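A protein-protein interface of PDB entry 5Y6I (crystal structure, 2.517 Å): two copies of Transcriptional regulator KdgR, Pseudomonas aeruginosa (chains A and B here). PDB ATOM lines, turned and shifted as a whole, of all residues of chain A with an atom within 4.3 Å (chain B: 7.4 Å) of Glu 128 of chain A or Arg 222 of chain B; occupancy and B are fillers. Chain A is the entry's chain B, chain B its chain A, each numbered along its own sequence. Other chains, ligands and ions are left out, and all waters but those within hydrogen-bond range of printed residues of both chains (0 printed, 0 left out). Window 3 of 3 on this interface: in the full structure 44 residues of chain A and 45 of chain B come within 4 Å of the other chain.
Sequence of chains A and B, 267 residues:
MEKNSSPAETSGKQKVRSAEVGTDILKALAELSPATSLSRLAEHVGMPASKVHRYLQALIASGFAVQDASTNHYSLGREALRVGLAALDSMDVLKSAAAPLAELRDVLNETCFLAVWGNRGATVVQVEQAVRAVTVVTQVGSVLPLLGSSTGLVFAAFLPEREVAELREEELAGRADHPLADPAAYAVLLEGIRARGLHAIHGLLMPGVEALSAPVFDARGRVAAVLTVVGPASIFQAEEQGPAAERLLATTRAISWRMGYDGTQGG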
ATOM      1  N   LEU A 101     -35.436  19.961  -1.113  1.00  0.00           N
ATOM      2  CA  LEU A 101     -35.323  18.687  -1.804  1.00  0.00           C
ATOM      3  C   LEU A 101     -33.918  18.132  -1.700  1.00  0.00           C
ATOM      4  O   LEU A 101     -33.744  16.911  -1.630  1.00  0.00           O
ATOM      5  CB  LEU A 101     -35.727  18.857  -3.270  1.00  0.00           C
ATOM      6  CG  LEU A 101     -35.692  17.625  -4.184  1.00  0.00           C
ATOM      7  CD1 LEU A 101     -36.688  16.577  -3.722  1.00  0.00           C
ATOM      8  CD2 LEU A 101     -35.928  18.000  -5.664  1.00  0.00           C
ATOM      9  N   ALA A 102     -32.906  19.006  -1.664  1.00  0.00           N
ATOM     10  CA  ALA A 102     -31.520  18.552  -1.608  1.00  0.00           C
ATOM     11  C   ALA A 102     -31.064  18.298  -0.176  1.00  0.00           C
ATOM     12  O   ALA A 102     -30.210  17.435   0.053  1.00  0.00           O
ATOM     13  CB  ALA A 102     -30.610  19.569  -2.294  1.00  0.00           C
ATOM     14  N   ARG A 105     -32.379  14.667   0.401  1.00  0.00           N
ATOM     15  CA  ARG A 105     -31.467  13.697  -0.192  1.00  0.00           C
ATOM     16  C   ARG A 105     -30.242  13.498   0.684  1.00  0.00           C
ATOM     17  O   ARG A 105     -29.787  12.364   0.894  1.00  0.00           O
ATOM     18  CB  ARG A 105     -31.043  14.169  -1.586  1.00  0.00           C
ATOM     19  CG  ARG A 105     -29.965  13.318  -2.261  1.00  0.00           C
ATOM     20  CD  ARG A 105     -28.507  13.773  -1.976  1.00  0.00           C
ATOM     21  NE  ARG A 105     -28.313  15.226  -1.927  1.00  0.00           N
ATOM     22  CZ  ARG A 105     -28.219  16.011  -2.999  1.00  0.00           C
ATOM     23  NH1 ARG A 105     -28.327  15.494  -4.220  1.00  0.00           N
ATOM     24  NH2 ARG A 105     -28.034  17.317  -2.847  1.00  0.00           N
ATOM     25  N   THR A 111     -32.086   8.849  -3.591  1.00  0.00           N
ATOM     26  CA  THR A 111     -32.468   9.860  -4.575  1.00  0.00           C
ATOM     27  C   THR A 111     -33.881  10.394  -4.308  1.00  0.00           C
ATOM     28  O   THR A 111     -34.822   9.633  -4.039  1.00  0.00           O
ATOM     29  CB  THR A 111     -32.388   9.275  -5.987  1.00  0.00           C
ATOM     30  OG1 THR A 111     -33.183   8.086  -6.038  1.00  0.00           O
ATOM     31  CG2 THR A 111     -30.938   8.899  -6.362  1.00  0.00           C
ATOM     32  N   CYS A 112     -34.027  11.717  -4.389  1.00  0.00           N
ATOM     33  CA  CYS A 112     -35.298  12.398  -4.187  1.00  0.00           C
ATOM     34  C   CYS A 112     -35.679  13.179  -5.435  1.00  0.00           C
ATOM     35  O   CYS A 112     -34.809  13.689  -6.146  1.00  0.00           O
ATOM     36  CB  CYS A 112     -35.235  13.374  -3.004  1.00  0.00           C
ATOM     37  SG  CYS A 112     -34.773  12.654  -1.429  1.00  0.00           S
ATOM     38  N   GLN A 126     -37.482  18.275 -10.926  1.00  0.00           N
ATOM     39  CA  GLN A 126     -36.151  18.382 -10.321  1.00  0.00           C
ATOM     40  C   GLN A 126     -35.781  17.060  -9.664  1.00  0.00           C
ATOM     41  O   GLN A 126     -36.592  16.482  -8.934  1.00  0.00           O
ATOM     42  CB  GLN A 126     -36.085  19.526  -9.292  1.00  0.00           C
ATOM     43  CG  GLN A 126     -34.753  19.658  -8.645  1.00  0.00           C
ATOM     44  CD  GLN A 126     -34.717  20.691  -7.507  1.00  0.00           C
ATOM     45  OE1 GLN A 126     -33.639  21.045  -7.007  1.00  0.00           O
ATOM     46  NE2 GLN A 126     -35.874  21.159  -7.091  1.00  0.00           N
ATOM     47  N   VAL A 127     -34.567  16.580  -9.927  1.00  0.00           N
ATOM     48  CA  VAL A 127     -34.082  15.308  -9.399  1.00  0.00           C
ATOM     49  C   VAL A 127     -32.775  15.552  -8.660  1.00  0.00           C
ATOM     50  O   VAL A 127     -31.801  16.015  -9.256  1.00  0.00           O
ATOM     51  CB  VAL A 127     -33.869  14.261 -10.507  1.00  0.00           C
ATOM     52  CG1 VAL A 127     -33.417  12.943  -9.896  1.00  0.00           C
ATOM     53  CG2 VAL A 127     -35.129  14.051 -11.297  1.00  0.00           C
ATOM     54  N   GLU A 128     -32.740  15.214  -7.372  1.00  0.00           N
ATOM     55  CA  GLU A 128     -31.519  15.306  -6.571  1.00  0.00           C
ATOM     56  C   GLU A 128     -31.081  13.888  -6.209  1.00  0.00           C
ATOM     57  O   GLU A 128     -31.735  13.212  -5.406  1.00  0.00           O
ATOM     58  CB  GLU A 128     -31.740  16.174  -5.331  1.00  0.00           C
ATOM     59  CG  GLU A 128     -32.043  17.645  -5.637  1.00  0.00           C
ATOM     60  CD  GLU A 128     -30.798  18.512  -5.766  1.00  0.00           C
ATOM     61  OE1 GLU A 128     -29.673  17.974  -5.631  1.00  0.00           O
ATOM     62  OE2 GLU A 128     -30.951  19.741  -5.983  1.00  0.00           O
ATOM     63  N   GLN A 129     -29.988  13.432  -6.811  1.00  0.00           N
ATOM     64  CA  GLN A 129     -29.567  12.048  -6.664  1.00  0.00           C
ATOM     65  C   GLN A 129     -28.485  11.912  -5.599  1.00  0.00           C
ATOM     66  O   GLN A 129     -27.688  12.823  -5.372  1.00  0.00           O
ATOM     67  CB  GLN A 129     -29.087  11.466  -7.998  1.00  0.00           C
ATOM     68  CG  GLN A 129     -27.857  12.112  -8.623  1.00  0.00           C
ATOM     69  CD  GLN A 129     -28.075  13.562  -9.047  1.00  0.00           C
ATOM     70  OE1 GLN A 129     -29.208  14.039  -9.143  1.00  0.00           O
ATOM     71  NE2 GLN A 129     -26.976  14.261  -9.327  1.00  0.00           N
ATOM     72  N   ALA A 130     -28.495  10.773  -4.917  1.00  0.00           N
ATOM     73  CA  ALA A 130     -27.539  10.537  -3.847  1.00  0.00           C
ATOM     74  C   ALA A 130     -26.176  10.262  -4.432  1.00  0.00           C
ATOM     75  O   ALA A 130     -26.057   9.808  -5.572  1.00  0.00           O
ATOM     76  CB  ALA A 130     -27.948   9.347  -2.978  1.00  0.00           C
ATOM     77  N   LEU B  88     -32.588  20.995 -19.026  1.00  0.00           N
ATOM     78  CA  LEU B  88     -32.047  20.661 -17.709  1.00  0.00           C
ATOM     79  C   LEU B  88     -31.762  19.164 -17.576  1.00  0.00           C
ATOM     80  O   LEU B  88     -30.824  18.762 -16.880  1.00  0.00           O
ATOM     81  CB  LEU B  88     -33.017  21.139 -16.624  1.00  0.00           C
ATOM     82  CG  LEU B  88     -33.209  22.662 -16.550  1.00  0.00           C
ATOM     83  CD1 LEU B  88     -34.541  22.991 -15.946  1.00  0.00           C
ATOM     84  CD2 LEU B  88     -32.116  23.316 -15.721  1.00  0.00           C
ATOM     85  N   MET B  91     -28.120  18.736 -19.199  1.00  0.00           N
ATOM     86  CA  MET B  91     -26.883  19.274 -18.649  1.00  0.00           C
ATOM     87  C   MET B  91     -25.867  18.158 -18.422  1.00  0.00           C
ATOM     88  O   MET B  91     -26.221  17.050 -18.009  1.00  0.00           O
ATOM     89  CB  MET B  91     -27.160  20.000 -17.336  1.00  0.00           C
ATOM     90  CG  MET B  91     -27.760  21.375 -17.452  1.00  0.00           C
ATOM     91  SD  MET B  91     -27.849  22.182 -15.836  1.00  0.00           S
ATOM     92  CE  MET B  91     -29.003  21.119 -14.986  1.00  0.00           C
ATOM     93  N   PHE B 158     -17.936  24.297  -0.805  1.00  0.00           N
ATOM     94  CA  PHE B 158     -19.180  24.576  -1.494  1.00  0.00           C
ATOM     95  C   PHE B 158     -20.265  23.521  -1.319  1.00  0.00           C
ATOM     96  O   PHE B 158     -21.441  23.867  -1.434  1.00  0.00           O
ATOM     97  CB  PHE B 158     -18.904  24.796  -2.983  1.00  0.00           C
ATOM     98  CG  PHE B 158     -18.203  26.087  -3.265  1.00  0.00           C
ATOM     99  CD1 PHE B 158     -16.822  26.169  -3.217  1.00  0.00           C
ATOM    100  CD2 PHE B 158     -18.931  27.242  -3.509  1.00  0.00           C
ATOM    101  CE1 PHE B 158     -16.172  27.369  -3.451  1.00  0.00           C
ATOM    102  CE2 PHE B 158     -18.285  28.448  -3.740  1.00  0.00           C
ATOM    103  CZ  PHE B 158     -16.899  28.508  -3.712  1.00  0.00           C
ATOM    104  N   LEU B 159     -19.937  22.273  -1.025  1.00  0.00           N
ATOM    105  CA  LEU B 159     -20.982  21.282  -0.810  1.00  0.00           C
ATOM    106  C   LEU B 159     -21.535  21.366   0.591  1.00  0.00           C
ATOM    107  O   LEU B 159     -20.898  21.893   1.508  1.00  0.00           O
ATOM    108  CB  LEU B 159     -20.464  19.876  -1.059  1.00  0.00           C
ATOM    109  CG  LEU B 159     -20.039  19.658  -2.486  1.00  0.00           C
ATOM    110  CD1 LEU B 159     -18.791  18.880  -2.430  1.00  0.00           C
ATOM    111  CD2 LEU B 159     -21.194  19.046  -3.338  1.00  0.00           C
ATOM    112  N   GLU B 163     -22.821  15.906   3.220  1.00  0.00           N
ATOM    113  CA  GLU B 163     -22.259  14.912   2.319  1.00  0.00           C
ATOM    114  C   GLU B 163     -20.731  14.938   2.260  1.00  0.00           C
ATOM    115  O   GLU B 163     -20.148  14.195   1.462  1.00  0.00           O
ATOM    116  CB  GLU B 163     -22.847  15.052   0.915  1.00  0.00           C
ATOM    117  CG  GLU B 163     -23.141  16.454   0.453  1.00  0.00           C
ATOM    118  CD  GLU B 163     -23.689  16.466  -0.965  1.00  0.00           C
ATOM    119  OE1 GLU B 163     -24.576  17.284  -1.263  1.00  0.00           O
ATOM    120  OE2 GLU B 163     -23.233  15.635  -1.778  1.00  0.00           O
ATOM    121  N   VAL B 216     -17.251  24.638 -10.553  1.00  0.00           N
ATOM    122  CA  VAL B 216     -18.149  24.764 -11.701  1.00  0.00           C
ATOM    123  C   VAL B 216     -19.576  24.434 -11.261  1.00  0.00           C
ATOM    124  O   VAL B 216     -19.813  23.392 -10.635  1.00  0.00           O
ATOM    125  CB  VAL B 216     -17.707  23.846 -12.855  1.00  0.00           C
ATOM    126  CG1 VAL B 216     -18.631  24.014 -14.043  1.00  0.00           C
ATOM    127  CG2 VAL B 216     -16.208  24.106 -13.224  1.00  0.00           C
ATOM    128  N   PHE B 217     -20.522  25.308 -11.611  1.00  0.00           N
ATOM    129  CA  PHE B 217     -21.906  25.242 -11.154  1.00  0.00           C
ATOM    130  C   PHE B 217     -22.848  24.884 -12.296  1.00  0.00           C
ATOM    131  O   PHE B 217     -22.589  25.212 -13.457  1.00  0.00           O
ATOM    132  CB  PHE B 217     -22.345  26.582 -10.567  1.00  0.00           C
ATOM    133  CG  PHE B 217     -21.485  27.057  -9.440  1.00  0.00           C
ATOM    134  CD1 PHE B 217     -21.650  26.541  -8.161  1.00  0.00           C
ATOM    135  CD2 PHE B 217     -20.504  28.010  -9.650  1.00  0.00           C
ATOM    136  CE1 PHE B 217     -20.842  26.978  -7.105  1.00  0.00           C
ATOM    137  CE2 PHE B 217     -19.696  28.449  -8.603  1.00  0.00           C
ATOM    138  CZ  PHE B 217     -19.867  27.938  -7.335  1.00  0.00           C
ATOM    139  N   ASP B 218     -23.971  24.244 -11.958  1.00  0.00           N
ATOM    140  CA  ASP B 218     -24.977  23.987 -12.974  1.00  0.00           C
ATOM    141  C   ASP B 218     -26.017  25.096 -12.948  1.00  0.00           C
ATOM    142  O   ASP B 218     -25.942  26.051 -12.162  1.00  0.00           O
ATOM    143  CB  ASP B 218     -25.602  22.591 -12.814  1.00  0.00           C
ATOM    144  CG  ASP B 218     -26.371  22.403 -11.509  1.00  0.00           C
ATOM    145  OD1 ASP B 218     -26.500  23.375 -10.714  1.00  0.00           O
ATOM    146  OD2 ASP B 218     -26.856  21.255 -11.276  1.00  0.00           O
ATOM    147  N   ALA B 219     -26.990  24.972 -13.860  1.00  0.00           N
ATOM    148  CA  ALA B 219     -28.088  25.926 -13.944  1.00  0.00           C
ATOM    149  C   ALA B 219     -28.677  26.238 -12.578  1.00  0.00           C
ATOM    150  O   ALA B 219     -29.016  27.393 -12.291  1.00  0.00           O
ATOM    151  CB  ALA B 219     -29.175  25.375 -14.869  1.00  0.00           C
ATOM    152  N   ARG B 220     -28.820  25.228 -11.720  1.00  0.00           N
ATOM    153  CA  ARG B 220     -29.494  25.437 -10.444  1.00  0.00           C
ATOM    154  C   ARG B 220     -28.538  25.871  -9.344  1.00  0.00           C
ATOM    155  O   ARG B 220     -28.961  26.013  -8.194  1.00  0.00           O
ATOM    156  CB  ARG B 220     -30.262  24.176 -10.036  1.00  0.00           C
ATOM    157  CG  ARG B 220     -30.928  23.476 -11.221  1.00  0.00           C
ATOM    158  CD  ARG B 220     -31.954  22.495 -10.753  1.00  0.00           C
ATOM    159  NE  ARG B 220     -32.761  23.158  -9.760  1.00  0.00           N
ATOM    160  CZ  ARG B 220     -34.072  23.344  -9.857  1.00  0.00           C
ATOM    161  NH1 ARG B 220     -34.754  22.866 -10.893  1.00  0.00           N
ATOM    162  NH2 ARG B 220     -34.701  23.986  -8.890  1.00  0.00           N
ATOM    163  N   GLY B 221     -27.277  26.115  -9.680  1.00  0.00           N
ATOM    164  CA  GLY B 221     -26.274  26.553  -8.737  1.00  0.00           C
ATOM    165  C   GLY B 221     -25.552  25.444  -8.009  1.00  0.00           C
ATOM    166  O   GLY B 221     -24.761  25.734  -7.094  1.00  0.00           O
ATOM    167  N   ARG B 222     -25.802  24.184  -8.361  1.00  0.00           N
ATOM    168  CA  ARG B 222     -25.223  23.072  -7.628  1.00  0.00           C
ATOM    169  C   ARG B 222     -23.811  22.852  -8.129  1.00  0.00           C
ATOM    170  O   ARG B 222     -23.514  23.076  -9.302  1.00  0.00           O
ATOM    171  CB  ARG B 222     -26.076  21.806  -7.802  1.00  0.00           C
ATOM    172  CG  ARG B 222     -27.599  22.051  -7.708  1.00  0.00           C
ATOM    173  CD  ARG B 222     -28.446  20.765  -7.792  1.00  0.00           C
ATOM    174  NE  ARG B 222     -28.477  20.196  -9.135  1.00  0.00           N
ATOM    175  CZ  ARG B 222     -29.505  19.528  -9.645  1.00  0.00           C
ATOM    176  NH1 ARG B 222     -30.599  19.358  -8.929  1.00  0.00           N
ATOM    177  NH2 ARG B 222     -29.445  19.052 -10.883  1.00  0.00           N
ATOM    178  N   VAL B 223     -22.916  22.449  -7.229  1.00  0.00           N
ATOM    179  CA  VAL B 223     -21.545  22.233  -7.660  1.00  0.00           C
ATOM    180  C   VAL B 223     -21.532  21.056  -8.618  1.00  0.00           C
ATOM    181  O   VAL B 223     -21.905  19.936  -8.250  1.00  0.00           O
ATOM    182  CB  VAL B 223     -20.610  22.004  -6.467  1.00  0.00           C
ATOM    183  CG1 VAL B 223     -19.206  21.732  -6.967  1.00  0.00           C
ATOM    184  CG2 VAL B 223     -20.617  23.222  -5.594  1.00  0.00           C
ATOM    185  N   ALA B 224     -21.125  21.313  -9.859  1.00  0.00           N
ATOM    186  CA  ALA B 224     -21.085  20.300 -10.904  1.00  0.00           C
ATOM    187  C   ALA B 224     -19.751  19.580 -10.925  1.00  0.00           C
ATOM    188  O   ALA B 224     -19.700  18.354 -11.086  1.00  0.00           O
ATOM    189  CB  ALA B 224     -21.327  20.940 -12.278  1.00  0.00           C
ATOM    190  N   ALA B 225     -18.679  20.343 -10.763  1.00  0.00           N
ATOM    191  CA  ALA B 225     -17.320  19.840 -10.839  1.00  0.00           C
ATOM    192  C   ALA B 225     -16.397  20.871 -10.200  1.00  0.00           C
ATOM    193  O   ALA B 225     -16.829  21.952  -9.781  1.00  0.00           O
ATOM    194  CB  ALA B 225     -16.916  19.553 -12.289  1.00  0.00           C
ATOM    195  N   SER B 256     -19.651  27.363 -16.467  1.00  0.00           N
ATOM    196  CA  SER B 256     -20.861  27.510 -15.675  1.00  0.00           C
ATOM    197  C   SER B 256     -21.962  28.156 -16.490  1.00  0.00           C
ATOM    198  O   SER B 256     -23.047  27.588 -16.656  1.00  0.00           O
ATOM    199  CB  SER B 256     -20.586  28.344 -14.423  1.00  0.00           C
ATOM    200  OG  SER B 256     -19.975  27.563 -13.417  1.00  0.00           O
ATOM    201  N   TYR B 261     -26.002  28.685 -15.488  1.00  0.00           N
ATOM    202  CA  TYR B 261     -25.815  29.323 -14.198  1.00  0.00           C
ATOM    203  C   TYR B 261     -25.755  30.827 -14.383  1.00  0.00           C
ATOM    204  O   TYR B 261     -25.043  31.322 -15.254  1.00  0.00           O
ATOM    205  CB  TYR B 261     -24.526  28.793 -13.552  1.00  0.00           C
ATOM    206  CG  TYR B 261     -24.239  29.410 -12.213  1.00  0.00           C
ATOM    207  CD1 TYR B 261     -25.145  29.291 -11.170  1.00  0.00           C
ATOM    208  CD2 TYR B 261     -23.068  30.123 -11.993  1.00  0.00           C
ATOM    209  CE1 TYR B 261     -24.898  29.861  -9.952  1.00  0.00           C
ATOM    210  CE2 TYR B 261     -22.805  30.691 -10.767  1.00  0.00           C
ATOM    211  CZ  TYR B 261     -23.730  30.565  -9.754  1.00  0.00           C
ATOM    212  OH  TYR B 261     -23.481  31.136  -8.525  1.00  0.00           O
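No position is printed for both chains. Of the 5 pairs that touch across the chains among the printed residues, none has its exchanged pair printed and touching as well.
NH1 of Arg 105 of chain A lies within salt-bridge range of OE1 of Glu 128 of chain A (3.2 Å). The backbone carbonyl oxygen of Gln 129 of chain A lies within hydrogen-bond range of the guanidinium group of Arg 105 of chain A (3.0 Å). The guanidinium group of Arg 222 of chain B is in salt-bridge range of the side-chain carboxylate of Asp 218 of chain B, at 2.9 Å. The backbone NH of Arg 105 of chain A is in hydrogen-bond range of the side-chain sulfur of Cys 112 of chain A, at 3.6 Å. The side-chain amide oxygen (OE1) of Gln 129 of chain A sits close to the backbone carbonyl oxygen (O) of Val 127 of chain A. O of Cys 112 of chain A sits at hydrogen-bond distance from N of Glu 128 of chain A (2.8 Å).
Among the printed residues, pairs that only touch across the chains: Gln 126 of chain A with Arg 220 of chain B (3.6 Å), Gln 126 of chain A with Arg 222 of chain B (3.97 Å) and Val 127 of chain A with Arg 222 of chain B (3.6 Å).
Of the 10 printed residues of chain A, 4 touch a printed residue of chain B. Printed residues of chain A that touch a printed residue of chain B: Arg 105, Gln 126, Val 127 and Glu 128. Printed residues of chain B that touch a printed residue of chain A: Glu 163, Arg 220 and Arg 222. Among the printed residues, 5 pairs touch across the chains. Among the printed residues, Asp or Glu carboxylates within 4 Å of a Lys or Arg side-chain nitrogen of the other chain: Arg 105 of chain A with Glu 163 of chain B and Glu 128 of chain A with Arg 222 of chain B.
The guanidinium group of Arg 222 of chain B lies within salt-bridge range of the side-chain carboxylate of Glu 128 of chain A. The guanidinium group (NH2) of Arg 105 of chain A lies within salt-bridge range of the side-chain carboxylate (OE1) of Glu 163 of chain B.
Glu 128 of chain A touches just one residue of chain B: Arg 222. Of chain A, only Gln 126, Val 127 and Glu 128 come within 4 Å of Arg 222 of chain B. Printed residues of chain A within 4 Å of Glu 163 of chain B: Arg 105. Of the printed residues of chain B, Arg 105 of chain A touches Glu 163. Of the printed residues of chain B, Gln 126 of chain A touches Arg 220 and Arg 222. Ser 256 of chain B touches none of the printed residues of chain A. Tyr 261 of chain B touches none of the printed residues of chain A.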
